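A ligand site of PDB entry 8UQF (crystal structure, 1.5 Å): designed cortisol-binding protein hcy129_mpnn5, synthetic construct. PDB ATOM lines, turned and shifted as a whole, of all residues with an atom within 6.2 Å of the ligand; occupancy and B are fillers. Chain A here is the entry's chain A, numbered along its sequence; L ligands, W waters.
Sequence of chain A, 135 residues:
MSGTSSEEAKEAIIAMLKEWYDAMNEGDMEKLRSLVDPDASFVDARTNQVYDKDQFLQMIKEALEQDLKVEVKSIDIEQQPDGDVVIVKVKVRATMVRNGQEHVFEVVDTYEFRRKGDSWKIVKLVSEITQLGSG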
ATOM      1  N   TRP A  20      11.875  25.359 -20.080  1.00  0.00           N
ATOM      2  CA  TRP A  20      10.692  25.013 -20.860  1.00  0.00           C
ATOM      3  C   TRP A  20      10.606  25.897 -22.102  1.00  0.00           C
ATOM      4  O   TRP A  20      10.520  25.408 -23.230  1.00  0.00           O
ATOM      5  CB  TRP A  20       9.430  25.179 -19.996  1.00  0.00           C
ATOM      6  CG  TRP A  20       8.141  24.918 -20.738  1.00  0.00           C
ATOM      7  CD1 TRP A  20       7.404  25.826 -21.440  1.00  0.00           C
ATOM      8  CD2 TRP A  20       7.492  23.646 -20.905  1.00  0.00           C
ATOM      9  NE1 TRP A  20       6.346  25.189 -22.060  1.00  0.00           N
ATOM     10  CE2 TRP A  20       6.378  23.849 -21.737  1.00  0.00           C
ATOM     11  CE3 TRP A  20       7.762  22.341 -20.453  1.00  0.00           C
ATOM     12  CZ2 TRP A  20       5.524  22.833 -22.107  1.00  0.00           C
ATOM     13  CZ3 TRP A  20       6.910  21.336 -20.809  1.00  0.00           C
ATOM     14  CH2 TRP A  20       5.792  21.578 -21.605  1.00  0.00           C
ATOM     15  N   TYR A  21      10.608  27.170 -21.876  1.00  0.00           N
ATOM     16  CA  TYR A  21      10.476  28.065 -22.969  1.00  0.00           C
ATOM     17  C   TYR A  21      11.701  28.040 -23.874  1.00  0.00           C
ATOM     18  O   TYR A  21      11.572  28.205 -25.029  1.00  0.00           O
ATOM     19  CB  TYR A  21      10.054  29.460 -22.479  1.00  0.00           C
ATOM     20  CG  TYR A  21       8.625  29.468 -21.915  1.00  0.00           C
ATOM     21  CD1 TYR A  21       7.537  29.384 -22.721  1.00  0.00           C
ATOM     22  CD2 TYR A  21       8.399  29.505 -20.586  1.00  0.00           C
ATOM     23  CE1 TYR A  21       6.271  29.366 -22.225  1.00  0.00           C
ATOM     24  CE2 TYR A  21       7.149  29.462 -20.103  1.00  0.00           C
ATOM     25  CZ  TYR A  21       6.125  29.472 -20.951  1.00  0.00           C
ATOM     26  OH  TYR A  21       4.864  29.357 -20.434  1.00  0.00           O
ATOM     27  N   MET A  24      11.362  25.116 -26.077  1.00  0.00           N
ATOM     28  CA  MET A  24      10.362  25.394 -27.059  1.00  0.00           C
ATOM     29  C   MET A  24      10.985  26.122 -28.233  1.00  0.00           C
ATOM     30  O   MET A  24      10.816  25.725 -29.316  1.00  0.00           O
ATOM     31  CB  MET A  24       9.235  26.219 -26.458  1.00  0.00           C
ATOM     32  CG  MET A  24       7.951  26.178 -27.226  1.00  0.00           C
ATOM     33  SD  MET A  24       7.098  24.584 -27.157  1.00  0.00           S
ATOM     34  CE  MET A  24       6.549  24.634 -25.455  1.00  0.00           C
ATOM     35  N   PHE A  42      -3.647  19.491 -19.146  1.00  0.00           N
ATOM     36  CA  PHE A  42      -3.425  20.721 -19.855  1.00  0.00           C
ATOM     37  C   PHE A  42      -4.726  21.330 -20.275  1.00  0.00           C
ATOM     38  O   PHE A  42      -5.436  20.727 -21.018  1.00  0.00           O
ATOM     39  CB  PHE A  42      -2.556  20.379 -21.048  1.00  0.00           C
ATOM     40  CG  PHE A  42      -1.213  19.972 -20.638  1.00  0.00           C
ATOM     41  CD1 PHE A  42      -0.880  18.692 -20.306  1.00  0.00           C
ATOM     42  CD2 PHE A  42      -0.327  20.914 -20.477  1.00  0.00           C
ATOM     43  CE1 PHE A  42       0.390  18.409 -19.876  1.00  0.00           C
ATOM     44  CE2 PHE A  42       0.933  20.681 -20.060  1.00  0.00           C
ATOM     45  CZ  PHE A  42       1.300  19.416 -19.766  1.00  0.00           C
ATOM     46  N   ASP A  44      -6.974  24.398 -22.089  1.00  0.00           N
ATOM     47  CA  ASP A  44      -7.158  25.566 -22.963  1.00  0.00           C
ATOM     48  C   ASP A  44      -8.318  26.325 -22.353  1.00  0.00           C
ATOM     49  O   ASP A  44      -9.469  25.917 -22.495  1.00  0.00           O
ATOM     50  CB  ASP A  44      -7.492  25.130 -24.384  1.00  0.00           C
ATOM     51  CG  ASP A  44      -7.533  26.279 -25.373  1.00  0.00           C
ATOM     52  OD1 ASP A  44      -7.948  27.376 -24.976  1.00  0.00           O
ATOM     53  OD2 ASP A  44      -7.198  26.020 -26.568  1.00  0.00           O
ATOM     54  N   PHE A  56      -1.215  16.847 -25.354  1.00  0.00           N
ATOM     55  CA  PHE A  56      -0.608  18.166 -25.302  1.00  0.00           C
ATOM     56  C   PHE A  56       0.671  18.204 -26.124  1.00  0.00           C
ATOM     57  O   PHE A  56       0.869  19.099 -26.951  1.00  0.00           O
ATOM     58  CB  PHE A  56      -0.311  18.538 -23.858  1.00  0.00           C
ATOM     59  CG  PHE A  56       0.428  19.867 -23.709  1.00  0.00           C
ATOM     60  CD1 PHE A  56      -0.232  21.083 -23.913  1.00  0.00           C
ATOM     61  CD2 PHE A  56       1.761  19.890 -23.324  1.00  0.00           C
ATOM     62  CE1 PHE A  56       0.469  22.288 -23.783  1.00  0.00           C
ATOM     63  CE2 PHE A  56       2.447  21.080 -23.174  1.00  0.00           C
ATOM     64  CZ  PHE A  56       1.791  22.279 -23.373  1.00  0.00           C
ATOM     65  N   MET A  59       0.146  18.314 -29.814  1.00  0.00           N
ATOM     66  CA  MET A  59      -0.197  19.652 -30.244  1.00  0.00           C
ATOM     67  C   MET A  59       1.020  20.519 -30.283  1.00  0.00           C
ATOM     68  O   MET A  59       1.153  21.301 -31.141  1.00  0.00           O
ATOM     69  CB  MET A  59      -1.287  20.249 -29.381  1.00  0.00           C
ATOM     70  CG  MET A  59      -2.600  19.581 -29.619  1.00  0.00           C
ATOM     71  SD  MET A  59      -3.948  20.340 -28.724  1.00  0.00           S
ATOM     72  CE  MET A  59      -3.590  22.012 -29.092  1.00  0.00           C
ATOM     73  N   ILE A  60       1.889  20.377 -29.303  1.00  0.00           N
ATOM     74  CA  ILE A  60       3.160  21.107 -29.350  1.00  0.00           C
ATOM     75  C   ILE A  60       3.941  20.727 -30.596  1.00  0.00           C
ATOM     76  O   ILE A  60       4.479  21.584 -31.284  1.00  0.00           O
ATOM     77  CB  ILE A  60       3.979  20.836 -28.081  1.00  0.00           C
ATOM     78  CG1 ILE A  60       3.281  21.478 -26.879  1.00  0.00           C
ATOM     79  CG2 ILE A  60       5.445  21.333 -28.221  1.00  0.00           C
ATOM     80  CD1 ILE A  60       3.136  23.007 -26.951  1.00  0.00           C
ATOM     81  N   ALA A  63       2.624  22.556 -33.523  1.00  0.00           N
ATOM     82  CA  ALA A  63       2.945  23.971 -33.474  1.00  0.00           C
ATOM     83  C   ALA A  63       4.405  24.218 -33.818  1.00  0.00           C
ATOM     84  O   ALA A  63       4.740  25.217 -34.474  1.00  0.00           O
ATOM     85  CB  ALA A  63       2.646  24.536 -32.097  1.00  0.00           C
ATOM     86  N   LEU A  68       6.644  27.624 -34.331  1.00  0.00           N
ATOM     87  CA  LEU A  68       6.327  28.283 -33.093  1.00  0.00           C
ATOM     88  C   LEU A  68       7.538  28.823 -32.386  1.00  0.00           C
ATOM     89  O   LEU A  68       8.486  28.127 -32.200  1.00  0.00           O
ATOM     90  CB  LEU A  68       5.603  27.308 -32.150  1.00  0.00           C
ATOM     91  CG  LEU A  68       5.377  27.768 -30.720  1.00  0.00           C
ATOM     92  CD1 LEU A  68       4.284  28.805 -30.726  1.00  0.00           C
ATOM     93  CD2 LEU A  68       5.024  26.605 -29.819  1.00  0.00           C
ATOM     94  N   LYS A  69       7.508  30.083 -32.025  1.00  0.00           N
ATOM     95  CA  LYS A  69       8.549  30.719 -31.235  1.00  0.00           C
ATOM     96  C   LYS A  69       7.902  31.480 -30.085  1.00  0.00           C
ATOM     97  O   LYS A  69       6.808  31.938 -30.200  1.00  0.00           O
ATOM     98  CB  LYS A  69       9.469  31.608 -32.057  1.00  0.00           C
ATOM     99  CG  LYS A  69      10.429  30.834 -32.953  1.00  0.00           C
ATOM    100  CD  LYS A  69      11.130  31.669 -34.014  1.00  0.00           C
ATOM    101  CE  LYS A  69      11.748  30.796 -35.107  1.00  0.00           C
ATOM    102  NZ  LYS A  69      12.439  31.512 -36.217  1.00  0.00           N
ATOM    103  N   VAL A  70       8.590  31.583 -28.979  1.00  0.00           N
ATOM    104  CA  VAL A  70       8.049  32.214 -27.805  1.00  0.00           C
ATOM    105  C   VAL A  70       9.048  33.137 -27.070  1.00  0.00           C
ATOM    106  O   VAL A  70      10.220  32.948 -27.171  1.00  0.00           O
ATOM    107  CB  VAL A  70       7.589  31.155 -26.793  1.00  0.00           C
ATOM    108  CG1 VAL A  70       6.409  30.320 -27.280  1.00  0.00           C
ATOM    109  CG2 VAL A  70       8.750  30.274 -26.413  1.00  0.00           C
ATOM    110  N   VAL A  92       3.466  35.287 -21.993  1.00  0.00           N
ATOM    111  CA  VAL A  92       4.318  34.993 -23.110  1.00  0.00           C
ATOM    112  C   VAL A  92       3.806  35.588 -24.435  1.00  0.00           C
ATOM    113  O   VAL A  92       2.627  35.655 -24.647  1.00  0.00           O
ATOM    114  CB  VAL A  92       4.302  33.458 -23.366  1.00  0.00           C
ATOM    115  CG1 VAL A  92       5.242  33.021 -24.448  1.00  0.00           C
ATOM    116  CG2 VAL A  92       4.557  32.656 -22.135  1.00  0.00           C
ATOM    117  N   ALA A  94       3.959  34.869 -28.431  1.00  0.00           N
ATOM    118  CA  ALA A  94       4.274  33.744 -29.291  1.00  0.00           C
ATOM    119  C   ALA A  94       3.950  34.074 -30.728  1.00  0.00           C
ATOM    120  O   ALA A  94       3.038  34.854 -31.017  1.00  0.00           O
ATOM    121  CB  ALA A  94       3.543  32.486 -28.881  1.00  0.00           C
ATOM    122  N   MET A  96       3.609  32.029 -34.713  1.00  0.00           N
ATOM    123  CA  MET A  96       3.526  30.823 -35.474  1.00  0.00           C
ATOM    124  C   MET A  96       3.343  31.230 -36.915  1.00  0.00           C
ATOM    125  O   MET A  96       2.688  32.184 -37.165  1.00  0.00           O
ATOM    126  CB  MET A  96       2.324  30.000 -35.073  1.00  0.00           C
ATOM    127  CG  MET A  96       2.671  28.842 -34.221  1.00  0.00           C
ATOM    128  SD  MET A  96       1.326  27.721 -33.957  1.00  0.00           S
ATOM    129  CE  MET A  96       0.011  28.860 -33.907  1.00  0.00           C
ATOM    130  N   PHE A 105       0.504  35.855 -30.865  1.00  0.00           N
ATOM    131  CA  PHE A 105      -0.306  35.590 -29.731  1.00  0.00           C
ATOM    132  C   PHE A 105       0.221  36.108 -28.404  1.00  0.00           C
ATOM    133  O   PHE A 105       1.385  36.255 -28.245  1.00  0.00           O
ATOM    134  CB  PHE A 105      -0.449  34.069 -29.539  1.00  0.00           C
ATOM    135  CG  PHE A 105      -0.903  33.347 -30.749  1.00  0.00           C
ATOM    136  CD1 PHE A 105      -0.013  32.992 -31.712  1.00  0.00           C
ATOM    137  CD2 PHE A 105      -2.216  33.011 -30.907  1.00  0.00           C
ATOM    138  CE1 PHE A 105      -0.413  32.347 -32.834  1.00  0.00           C
ATOM    139  CE2 PHE A 105      -2.615  32.366 -32.029  1.00  0.00           C
ATOM    140  CZ  PHE A 105      -1.711  32.013 -32.995  1.00  0.00           C
ATOM    141  N   VAL A 107      -0.107  34.887 -24.503  1.00  0.00           N
ATOM    142  CA  VAL A 107      -0.589  33.741 -23.755  1.00  0.00           C
ATOM    143  C   VAL A 107      -0.289  33.939 -22.284  1.00  0.00           C
ATOM    144  O   VAL A 107       0.809  34.342 -21.909  1.00  0.00           O
ATOM    145  CB  VAL A 107       0.073  32.434 -24.263  1.00  0.00           C
ATOM    146  CG1 VAL A 107      -0.506  31.287 -23.465  1.00  0.00           C
ATOM    147  CG2 VAL A 107      -0.223  32.265 -25.791  1.00  0.00           C
ATOM    148  N   ASP A 109       0.069  31.664 -19.152  1.00  0.00           N
ATOM    149  CA  ASP A 109       0.239  30.265 -18.747  1.00  0.00           C
ATOM    150  C   ASP A 109       0.298  30.216 -17.235  1.00  0.00           C
ATOM    151  O   ASP A 109       1.191  30.809 -16.626  1.00  0.00           O
ATOM    152  CB  ASP A 109       1.535  29.703 -19.318  1.00  0.00           C
ATOM    153  CG  ASP A 109       1.410  29.331 -20.779  1.00  0.00           C
ATOM    154  OD1 ASP A 109       0.315  28.956 -21.212  1.00  0.00           O
ATOM    155  OD2 ASP A 109       2.458  29.409 -21.498  1.00  0.00           O
ATOM    156  N   TYR A 111       0.833  27.615 -14.299  1.00  0.00           N
ATOM    157  CA  TYR A 111       1.348  26.290 -14.003  1.00  0.00           C
ATOM    158  C   TYR A 111       1.113  25.944 -12.550  1.00  0.00           C
ATOM    159  O   TYR A 111       1.317  26.790 -11.685  1.00  0.00           O
ATOM    160  CB  TYR A 111       2.865  26.203 -14.225  1.00  0.00           C
ATOM    161  CG  TYR A 111       3.292  26.361 -15.667  1.00  0.00           C
ATOM    162  CD1 TYR A 111       3.497  27.603 -16.224  1.00  0.00           C
ATOM    163  CD2 TYR A 111       3.439  25.255 -16.482  1.00  0.00           C
ATOM    164  CE1 TYR A 111       3.878  27.726 -17.576  1.00  0.00           C
ATOM    165  CE2 TYR A 111       3.815  25.380 -17.821  1.00  0.00           C
ATOM    166  CZ  TYR A 111       4.030  26.623 -18.337  1.00  0.00           C
ATOM    167  OH  TYR A 111       4.393  26.784 -19.650  1.00  0.00           O
ATOM    168  N   LEU A 125      -1.397  22.689 -16.324  1.00  0.00           N
ATOM    169  CA  LEU A 125      -1.218  23.999 -16.949  1.00  0.00           C
ATOM    170  C   LEU A 125      -2.566  24.497 -17.447  1.00  0.00           C
ATOM    171  O   LEU A 125      -3.272  23.767 -18.126  1.00  0.00           O
ATOM    172  CB  LEU A 125      -0.249  23.924 -18.114  1.00  0.00           C
ATOM    173  CG  LEU A 125      -0.274  25.085 -19.092  1.00  0.00           C
ATOM    174  CD1 LEU A 125       0.150  26.396 -18.440  1.00  0.00           C
ATOM    175  CD2 LEU A 125       0.583  24.728 -20.287  1.00  0.00           C
ATOM    176  N   SER A 127      -3.848  27.541 -19.959  1.00  0.00           N
ATOM    177  CA  SER A 127      -3.366  28.549 -20.908  1.00  0.00           C
ATOM    178  C   SER A 127      -4.502  29.412 -21.465  1.00  0.00           C
ATOM    179  O   SER A 127      -5.421  28.888 -22.021  1.00  0.00           O
ATOM    180  CB  SER A 127      -2.688  27.897 -22.107  1.00  0.00           C
ATOM    181  OG  SER A 127      -1.699  27.006 -21.747  1.00  0.00           O
ATOM    182  N   ILE A 129      -5.146  31.884 -24.292  1.00  0.00           N
ATOM    183  CA  ILE A 129      -4.501  32.209 -25.555  1.00  0.00           C
ATOM    184  C   ILE A 129      -5.319  33.267 -26.291  1.00  0.00           C
ATOM    185  O   ILE A 129      -6.489  33.034 -26.587  1.00  0.00           O
ATOM    186  CB  ILE A 129      -4.362  30.957 -26.428  1.00  0.00           C
ATOM    187  CG1 ILE A 129      -3.467  29.954 -25.706  1.00  0.00           C
ATOM    188  CG2 ILE A 129      -3.800  31.362 -27.803  1.00  0.00           C
ATOM    189  CD1 ILE A 129      -3.694  28.533 -26.102  1.00  0.00           C
HETATM  190  C1  LIG L   1      -2.351  26.193 -29.201  1.00  0.00           C
HETATM  191  C2  LIG L   1      -3.175  26.233 -30.054  1.00  0.00           C
HETATM  192  C3  LIG L   1      -3.504  27.752 -30.590  1.00  0.00           C
HETATM  193  C4  LIG L   1      -2.425  28.758 -30.597  1.00  0.00           C
HETATM  194  C5  LIG L   1      -1.143  28.364 -30.065  1.00  0.00           C
HETATM  195  C6  LIG L   1       0.113  29.387 -30.029  1.00  0.00           C
HETATM  196  C7  LIG L   1       0.659  29.538 -28.723  1.00  0.00           C
HETATM  197  C8  LIG L   1       0.985  28.267 -28.145  1.00  0.00           C
HETATM  198  C9  LIG L   1      -0.251  27.326 -28.137  1.00  0.00           C
HETATM  199  C10 LIG L   1      -0.857  27.128 -29.507  1.00  0.00           C
HETATM  200  C11 LIG L   1       0.668  26.298 -25.851  1.00  0.00           C
HETATM  201  C12 LIG L   1       0.057  25.955 -27.302  1.00  0.00           C
HETATM  202  C13 LIG L   1       1.918  27.200 -25.855  1.00  0.00           C
HETATM  203  C14 LIG L   1       1.537  28.572 -26.722  1.00  0.00           C
HETATM  204  C15 LIG L   1       2.595  29.393 -26.533  1.00  0.00           C
HETATM  205  C16 LIG L   1       3.171  29.008 -25.090  1.00  0.00           C
HETATM  206  C17 LIG L   1       2.184  27.879 -24.747  1.00  0.00           C
HETATM  207  C18 LIG L   1       3.148  26.491 -26.512  1.00  0.00           C
HETATM  208  C19 LIG L   1       0.066  26.322 -30.425  1.00  0.00           C
HETATM  209  C20 LIG L   1       3.138  26.979 -23.843  1.00  0.00           C
HETATM  210  C21 LIG L   1       2.484  26.044 -22.830  1.00  0.00           C
HETATM  211  O1  LIG L   1      -4.555  28.056 -30.980  1.00  0.00           O
HETATM  212  O2  LIG L   1       0.843  25.163 -27.989  1.00  0.00           O
HETATM  213  O3  LIG L   1       1.185  28.149 -23.858  1.00  0.00           O
HETATM  214  O4  LIG L   1       4.290  26.991 -23.814  1.00  0.00           O
HETATM  215  O5  LIG L   1       3.424  25.298 -22.044  1.00  0.00           O
HETATM  216  O   HOH W   1      -0.169  22.746 -26.949  1.00  0.00           O
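O5 of the ligand sits at hydrogen-bond distance from OH of Tyr 111.
The side-chain carboxylate (OD1) of Asp 109 sits at hydrogen-bond distance from an oxygen (O3) of the ligand.
The indole nitrogen (NE1) of Trp 20 lies within hydrogen-bond range of an oxygen (O5) of the ligand, 2.9 Å away.
The side-chain hydroxyl (OH) of Tyr 21 lies within hydrogen-bond range of the side-chain carboxylate (OD2) of Asp 109 (2.6 Å).
The side-chain hydroxyl (OH) of Tyr 111 is in hydrogen-bond range of the indole nitrogen (NE1) of Trp 20.
N of Val 92 sits at hydrogen-bond distance from O of Val 107 (2.8 Å).
The backbone NH (N) of Phe 105 lies within hydrogen-bond range of the backbone carbonyl oxygen (O) of Ala 94 (2.7 Å).
OD1 of Asp 109 sits at hydrogen-bond distance from OG of Ser 127, 2.9 Å away.
N of Leu 68 lies within hydrogen-bond range of O of Ala 63 (3.1 Å).
The side-chain hydroxyl (OH) of Tyr 21 lies within hydrogen-bond range of the side-chain hydroxyl (OH) of Tyr 111.
CE1 of Tyr 21 touches O4 of the ligand, at 3.5 Å.
Met 24 touches the ligand (CE to O4, 3.7 Å).
Phe 56 touches the ligand.
CD1 of Ile 60 touches O2 of the ligand, at 3.3 Å.
Ala 63 touches the ligand.
Leu 68 touches the ligand.
Val 70 touches the ligand (CG1 to C15, 3.995 Å).
Ala 94 touches the ligand (CB to C15, 3.997 Å).
Met 96 touches the ligand (CE to C6, 3.9 Å).
Phe 105 touches the ligand.
CG1 of Val 107 touches O3 of the ligand, at 3.6 Å.
Leu 125 touches the ligand (CD2 to O5, 3.4 Å).
Ser 127 touches the ligand (OG to O3, 3.8 Å).
Hydrophobic or aromatic side chains that line the ligand: Trp 20, Tyr 21, Met 24, Phe 56, Ile 60, Ala 63, Leu 68, Val 70, Ala 94, Met 96, Phe 105, Val 107, Tyr 111 and Leu 125.
The nearest printed residue that does not touch the ligand is Ile 129 (4.1 Å).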
